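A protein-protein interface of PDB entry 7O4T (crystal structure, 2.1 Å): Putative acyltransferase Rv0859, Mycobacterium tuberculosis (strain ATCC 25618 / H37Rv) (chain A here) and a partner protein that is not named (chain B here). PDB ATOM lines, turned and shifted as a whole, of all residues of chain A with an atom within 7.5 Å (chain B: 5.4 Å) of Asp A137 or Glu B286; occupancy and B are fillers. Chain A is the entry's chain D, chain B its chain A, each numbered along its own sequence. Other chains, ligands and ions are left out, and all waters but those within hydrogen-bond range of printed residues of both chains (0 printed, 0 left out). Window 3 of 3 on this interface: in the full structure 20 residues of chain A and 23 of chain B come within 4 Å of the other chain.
Glu B286 touches Asp A137.
CA of Pro A138 touches CG of Pro B262 (3.7 Å).
Leu B281 touches Pro A138 (CG to CB, 3.8 Å).
Pro A138 touches Val B285 (CG to CG2, 3.6 Å).
Tyr B302 touches Ala A139.
Pro B262 touches Asn A141 (CG to CG, 3.7 Å).
Of the 13 printed residues of chain A, 4 touch a printed residue of chain B.
Printed residues of chain B that touch a printed residue of chain A: Pro B262, Leu B281, Val B285, Glu B286 and Tyr B302.
Hydrophobic or aromatic side chains of chain B that line the printed part of chain A: Pro B262, Leu B281, Val B285 and Tyr B302.
Among the printed residues, 6 pairs touch across the chains.
Printed residues of chain B within 4 Å of Asp A137: Glu B286 (3.99 Å).
Printed residues of chain A within 4 Å of Glu B286: Asp A137 (3.99 Å).
Of the printed residues of chain A, Val B285 touches Pro A138.
Printed residues of chain B within 4 Å of Asn A141: Pro B262.
The nearest printed residue of chain B that does not touch Asp A137 is Pro B262 (5.1 Å).
The nearest printed residue of chain B that does not touch Asn A141 is Leu B281 (7.5 Å).
The side-chain carboxylate (OE2) of Glu B286 is in hydrogen-bond range of the side-chain hydroxyl (OH) of Tyr B302, 2.4 Å away.
The side-chain amide nitrogen (ND2) of Asn A141 is in hydrogen-bond range of the backbone carbonyl oxygen (O) of Gly A135 (2.9 Å).
OD2 of Asp A137 sits at hydrogen-bond distance from OG1 of Thr A140, at 2.8 Å.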
ATOM      1  N   GLY A 132      25.992  17.189 -35.801  1.00  0.00           N
ATOM      2  CA  GLY A 132      26.922  17.648 -34.785  1.00  0.00           C
ATOM      3  C   GLY A 132      26.271  17.668 -33.415  1.00  0.00           C
ATOM      4  O   GLY A 132      25.049  17.663 -33.272  1.00  0.00           O
ATOM      5  N   ALA A 133      27.116  17.699 -32.381  1.00  0.00           N
ATOM      6  CA  ALA A 133      26.616  17.669 -31.009  1.00  0.00           C
ATOM      7  C   ALA A 133      26.211  19.056 -30.519  1.00  0.00           C
ATOM      8  O   ALA A 133      25.179  19.201 -29.854  1.00  0.00           O
ATOM      9  CB  ALA A 133      27.667  17.067 -30.079  1.00  0.00           C
ATOM     10  N   MET A 134      27.008  20.081 -30.831  1.00  0.00           N
ATOM     11  CA  MET A 134      26.701  21.436 -30.380  1.00  0.00           C
ATOM     12  C   MET A 134      25.335  21.914 -30.851  1.00  0.00           C
ATOM     13  O   MET A 134      24.760  22.819 -30.236  1.00  0.00           O
ATOM     14  CB  MET A 134      27.780  22.411 -30.859  1.00  0.00           C
ATOM     15  CG  MET A 134      29.123  22.249 -30.162  1.00  0.00           C
ATOM     16  SD  MET A 134      30.367  23.409 -30.770  1.00  0.00           S
ATOM     17  CE  MET A 134      30.563  22.844 -32.459  1.00  0.00           C
ATOM     18  N   GLY A 135      24.799  21.327 -31.919  1.00  0.00           N
ATOM     19  CA  GLY A 135      23.496  21.718 -32.412  1.00  0.00           C
ATOM     20  C   GLY A 135      22.410  20.695 -32.141  1.00  0.00           C
ATOM     21  O   GLY A 135      21.319  21.052 -31.690  1.00  0.00           O
ATOM     22  N   LEU A 136      22.699  19.420 -32.398  1.00  0.00           N
ATOM     23  CA  LEU A 136      21.690  18.366 -32.374  1.00  0.00           C
ATOM     24  C   LEU A 136      21.806  17.470 -31.141  1.00  0.00           C
ATOM     25  O   LEU A 136      21.438  16.293 -31.187  1.00  0.00           O
ATOM     26  CB  LEU A 136      21.764  17.531 -33.651  1.00  0.00           C
ATOM     27  CG  LEU A 136      21.543  18.256 -34.985  1.00  0.00           C
ATOM     28  CD1 LEU A 136      22.841  18.841 -35.532  1.00  0.00           C
ATOM     29  CD2 LEU A 136      20.901  17.326 -36.002  1.00  0.00           C
ATOM     30  N   ASP A 137      22.315  18.009 -30.035  1.00  0.00           N
ATOM     31  CA  ASP A 137      22.313  17.303 -28.758  1.00  0.00           C
ATOM     32  C   ASP A 137      21.860  18.263 -27.665  1.00  0.00           C
ATOM     33  O   ASP A 137      22.595  19.197 -27.318  1.00  0.00           O
ATOM     34  CB  ASP A 137      23.695  16.729 -28.439  1.00  0.00           C
ATOM     35  CG  ASP A 137      23.737  16.039 -27.090  1.00  0.00           C
ATOM     36  OD1 ASP A 137      23.018  15.035 -26.915  1.00  0.00           O
ATOM     37  OD2 ASP A 137      24.487  16.500 -26.203  1.00  0.00           O
ATOM     38  N   PRO A 138      20.662  18.065 -27.103  1.00  0.00           N
ATOM     39  CA  PRO A 138      20.091  19.096 -26.219  1.00  0.00           C
ATOM     40  C   PRO A 138      20.948  19.421 -25.011  1.00  0.00           C
ATOM     41  O   PRO A 138      21.106  20.604 -24.678  1.00  0.00           O
ATOM     42  CB  PRO A 138      18.739  18.491 -25.812  1.00  0.00           C
ATOM     43  CG  PRO A 138      18.405  17.547 -26.915  1.00  0.00           C
ATOM     44  CD  PRO A 138      19.722  16.961 -27.343  1.00  0.00           C
ATOM     45  N   ALA A 139      21.511  18.412 -24.342  1.00  0.00           N
ATOM     46  CA  ALA A 139      22.338  18.676 -23.168  1.00  0.00           C
ATOM     47  C   ALA A 139      23.533  19.557 -23.519  1.00  0.00           C
ATOM     48  O   ALA A 139      23.872  20.481 -22.771  1.00  0.00           O
ATOM     49  CB  ALA A 139      22.806  17.361 -22.546  1.00  0.00           C
ATOM     50  N   THR A 140      24.180  19.290 -24.654  1.00  0.00           N
ATOM     51  CA  THR A 140      25.326  20.098 -25.059  1.00  0.00           C
ATOM     52  C   THR A 140      24.879  21.458 -25.582  1.00  0.00           C
ATOM     53  O   THR A 140      25.443  22.493 -25.210  1.00  0.00           O
ATOM     54  CB  THR A 140      26.147  19.355 -26.115  1.00  0.00           C
ATOM     55  OG1 THR A 140      26.700  18.161 -25.542  1.00  0.00           O
ATOM     56  CG2 THR A 140      27.273  20.234 -26.640  1.00  0.00           C
ATOM     57  N   ASN A 141      23.863  21.466 -26.452  1.00  0.00           N
ATOM     58  CA  ASN A 141      23.308  22.715 -26.966  1.00  0.00           C
ATOM     59  C   ASN A 141      22.915  23.652 -25.831  1.00  0.00           C
ATOM     60  O   ASN A 141      23.188  24.857 -25.883  1.00  0.00           O
ATOM     61  CB  ASN A 141      22.101  22.402 -27.857  1.00  0.00           C
ATOM     62  CG  ASN A 141      21.595  23.612 -28.633  1.00  0.00           C
ATOM     63  OD1 ASN A 141      21.491  24.719 -28.104  1.00  0.00           O
ATOM     64  ND2 ASN A 141      21.262  23.393 -29.900  1.00  0.00           N
ATOM     65  N   TYR A 142      22.284  23.107 -24.787  1.00  0.00           N
ATOM     66  CA  TYR A 142      21.794  23.929 -23.685  1.00  0.00           C
ATOM     67  C   TYR A 142      22.942  24.600 -22.943  1.00  0.00           C
ATOM     68  O   TYR A 142      22.883  25.797 -22.634  1.00  0.00           O
ATOM     69  CB  TYR A 142      20.971  23.063 -22.730  1.00  0.00           C
ATOM     70  CG  TYR A 142      19.936  23.805 -21.915  1.00  0.00           C
ATOM     71  CD1 TYR A 142      20.293  24.505 -20.769  1.00  0.00           C
ATOM     72  CD2 TYR A 142      18.594  23.780 -22.278  1.00  0.00           C
ATOM     73  CE1 TYR A 142      19.345  25.174 -20.016  1.00  0.00           C
ATOM     74  CE2 TYR A 142      17.638  24.444 -21.532  1.00  0.00           C
ATOM     75  CZ  TYR A 142      18.017  25.137 -20.402  1.00  0.00           C
ATOM     76  OH  TYR A 142      17.068  25.797 -19.656  1.00  0.00           O
ATOM     77  N   ASP A 143      24.001  23.845 -22.650  1.00  0.00           N
ATOM     78  CA  ASP A 143      25.100  24.380 -21.853  1.00  0.00           C
ATOM     79  C   ASP A 143      25.984  25.320 -22.663  1.00  0.00           C
ATOM     80  O   ASP A 143      26.358  26.392 -22.177  1.00  0.00           O
ATOM     81  CB  ASP A 143      25.929  23.233 -21.271  1.00  0.00           C
ATOM     82  CG  ASP A 143      25.097  22.278 -20.438  1.00  0.00           C
ATOM     83  OD1 ASP A 143      24.024  22.690 -19.948  1.00  0.00           O
ATOM     84  OD2 ASP A 143      25.515  21.113 -20.273  1.00  0.00           O
ATOM     85  N   VAL A 144      26.325  24.940 -23.897  1.00  0.00           N
ATOM     86  CA  VAL A 144      27.174  25.774 -24.741  1.00  0.00           C
ATOM     87  C   VAL A 144      26.479  27.047 -25.199  1.00  0.00           C
ATOM     88  O   VAL A 144      27.144  27.951 -25.719  1.00  0.00           O
ATOM     89  CB  VAL A 144      27.660  24.969 -25.965  1.00  0.00           C
ATOM     90  CG1 VAL A 144      26.590  24.937 -27.047  1.00  0.00           C
ATOM     91  CG2 VAL A 144      28.953  25.539 -26.505  1.00  0.00           C
ATOM     92  N   PRO B 262      16.426  23.208 -27.829  1.00  0.00           N
ATOM     93  CA  PRO B 262      16.989  23.694 -26.559  1.00  0.00           C
ATOM     94  C   PRO B 262      16.955  25.204 -26.431  1.00  0.00           C
ATOM     95  O   PRO B 262      16.794  25.711 -25.314  1.00  0.00           O
ATOM     96  CB  PRO B 262      18.431  23.163 -26.580  1.00  0.00           C
ATOM     97  CG  PRO B 262      18.434  22.079 -27.602  1.00  0.00           C
ATOM     98  CD  PRO B 262      17.448  22.513 -28.631  1.00  0.00           C
ATOM     99  N   LEU B 281      14.201  16.846 -22.151  1.00  0.00           N
ATOM    100  CA  LEU B 281      14.499  17.004 -23.571  1.00  0.00           C
ATOM    101  C   LEU B 281      15.697  16.156 -23.977  1.00  0.00           C
ATOM    102  O   LEU B 281      15.678  15.487 -25.017  1.00  0.00           O
ATOM    103  CB  LEU B 281      14.748  18.477 -23.893  1.00  0.00           C
ATOM    104  CG  LEU B 281      15.003  18.815 -25.363  1.00  0.00           C
ATOM    105  CD1 LEU B 281      13.809  18.414 -26.218  1.00  0.00           C
ATOM    106  CD2 LEU B 281      15.310  20.294 -25.526  1.00  0.00           C
ATOM    107  N   ALA B 282      16.753  16.171 -23.158  1.00  0.00           N
ATOM    108  CA  ALA B 282      17.933  15.363 -23.450  1.00  0.00           C
ATOM    109  C   ALA B 282      17.582  13.881 -23.505  1.00  0.00           C
ATOM    110  O   ALA B 282      17.977  13.173 -24.439  1.00  0.00           O
ATOM    111  CB  ALA B 282      19.020  15.623 -22.405  1.00  0.00           C
ATOM    112  N   ALA B 283      16.825  13.398 -22.515  1.00  0.00           N
ATOM    113  CA  ALA B 283      16.454  11.985 -22.488  1.00  0.00           C
ATOM    114  C   ALA B 283      15.596  11.614 -23.690  1.00  0.00           C
ATOM    115  O   ALA B 283      15.751  10.527 -24.261  1.00  0.00           O
ATOM    116  CB  ALA B 283      15.723  11.654 -21.187  1.00  0.00           C
ATOM    117  N   ALA B 284      14.683  12.503 -24.089  1.00  0.00           N
ATOM    118  CA  ALA B 284      13.819  12.218 -25.229  1.00  0.00           C
ATOM    119  C   ALA B 284      14.625  12.101 -26.517  1.00  0.00           C
ATOM    120  O   ALA B 284      14.455  11.149 -27.287  1.00  0.00           O
ATOM    121  CB  ALA B 284      12.748  13.304 -25.358  1.00  0.00           C
ATOM    122  N   VAL B 285      15.518  13.060 -26.764  1.00  0.00           N
ATOM    123  CA  VAL B 285      16.283  13.065 -28.009  1.00  0.00           C
ATOM    124  C   VAL B 285      17.308  11.936 -28.016  1.00  0.00           C
ATOM    125  O   VAL B 285      17.421  11.187 -28.994  1.00  0.00           O
ATOM    126  CB  VAL B 285      16.948  14.436 -28.221  1.00  0.00           C
ATOM    127  CG1 VAL B 285      17.926  14.382 -29.388  1.00  0.00           C
ATOM    128  CG2 VAL B 285      15.885  15.503 -28.458  1.00  0.00           C
ATOM    129  N   GLU B 286      18.078  11.801 -26.932  1.00  0.00           N
ATOM    130  CA  GLU B 286      19.069  10.729 -26.860  1.00  0.00           C
ATOM    131  C   GLU B 286      18.408   9.362 -26.963  1.00  0.00           C
ATOM    132  O   GLU B 286      18.947   8.448 -27.597  1.00  0.00           O
ATOM    133  CB  GLU B 286      19.872  10.828 -25.564  1.00  0.00           C
ATOM    134  CG  GLU B 286      20.766  12.053 -25.457  1.00  0.00           C
ATOM    135  CD  GLU B 286      21.519  12.102 -24.139  1.00  0.00           C
ATOM    136  OE1 GLU B 286      21.888  11.024 -23.626  1.00  0.00           O
ATOM    137  OE2 GLU B 286      21.731  13.215 -23.611  1.00  0.00           O
ATOM    138  N   GLY B 287      17.233   9.205 -26.350  1.00  0.00           N
ATOM    139  CA  GLY B 287      16.534   7.936 -26.432  1.00  0.00           C
ATOM    140  C   GLY B 287      16.055   7.610 -27.832  1.00  0.00           C
ATOM    141  O   GLY B 287      15.995   6.438 -28.213  1.00  0.00           O
ATOM    142  N   ALA B 288      15.712   8.633 -28.616  1.00  0.00           N
ATOM    143  CA  ALA B 288      15.252   8.415 -29.982  1.00  0.00           C
ATOM    144  C   ALA B 288      16.376   8.015 -30.928  1.00  0.00           C
ATOM    145  O   ALA B 288      16.092   7.631 -32.066  1.00  0.00           O
ATOM    146  CB  ALA B 288      14.556   9.671 -30.509  1.00  0.00           C
ATOM    147  N   GLN B 289      17.634   8.092 -30.492  1.00  0.00           N
ATOM    148  CA  GLN B 289      18.762   7.711 -31.332  1.00  0.00           C
ATOM    149  C   GLN B 289      19.116   6.234 -31.231  1.00  0.00           C
ATOM    150  O   GLN B 289      19.847   5.728 -32.092  1.00  0.00           O
ATOM    151  CB  GLN B 289      19.999   8.539 -30.968  1.00  0.00           C
ATOM    152  CG  GLN B 289      19.851  10.033 -31.188  1.00  0.00           C
ATOM    153  CD  GLN B 289      21.127  10.787 -30.867  1.00  0.00           C
ATOM    154  OE1 GLN B 289      21.417  11.077 -29.706  1.00  0.00           O
ATOM    155  NE2 GLN B 289      21.905  11.101 -31.898  1.00  0.00           N
ATOM    156  N   VAL B 290      18.618   5.531 -30.215  1.00  0.00           N
ATOM    157  CA  VAL B 290      19.027   4.169 -29.922  1.00  0.00           C
ATOM    158  C   VAL B 290      17.785   3.291 -29.795  1.00  0.00           C
ATOM    159  O   VAL B 290      16.651   3.764 -29.874  1.00  0.00           O
ATOM    160  CB  VAL B 290      19.889   4.084 -28.646  1.00  0.00           C
ATOM    161  CG1 VAL B 290      21.232   4.768 -28.866  1.00  0.00           C
ATOM    162  CG2 VAL B 290      19.152   4.716 -27.474  1.00  0.00           C
ATOM    163  N   ILE B 298      18.991   5.077 -20.538  1.00  0.00           N
ATOM    164  CA  ILE B 298      19.366   6.491 -20.539  1.00  0.00           C
ATOM    165  C   ILE B 298      18.378   7.304 -19.714  1.00  0.00           C
ATOM    166  O   ILE B 298      18.765   8.183 -18.934  1.00  0.00           O
ATOM    167  CB  ILE B 298      19.455   7.016 -21.983  1.00  0.00           C
ATOM    168  CG1 ILE B 298      20.611   6.353 -22.734  1.00  0.00           C
ATOM    169  CG2 ILE B 298      19.591   8.532 -21.996  1.00  0.00           C
ATOM    170  CD1 ILE B 298      20.660   6.722 -24.205  1.00  0.00           C
ATOM    171  N   TYR B 302      19.089  10.005 -16.333  1.00  0.00           N
ATOM    172  CA  TYR B 302      18.620  11.372 -16.138  1.00  0.00           C
ATOM    173  C   TYR B 302      17.658  11.473 -14.962  1.00  0.00           C
ATOM    174  O   TYR B 302      17.630  12.500 -14.276  1.00  0.00           O
ATOM    175  CB  TYR B 302      17.967  11.899 -17.416  1.00  0.00           C
ATOM    176  CG  TYR B 302      18.969  12.392 -18.439  1.00  0.00           C
ATOM    177  CD1 TYR B 302      19.638  13.594 -18.256  1.00  0.00           C
ATOM    178  CD2 TYR B 302      19.247  11.654 -19.582  1.00  0.00           C
ATOM    179  CE1 TYR B 302      20.559  14.052 -19.186  1.00  0.00           C
ATOM    180  CE2 TYR B 302      20.167  12.103 -20.519  1.00  0.00           C
ATOM    181  CZ  TYR B 302      20.819  13.302 -20.315  1.00  0.00           C
ATOM    182  OH  TYR B 302      21.731  13.752 -21.243  1.00  0.00           O
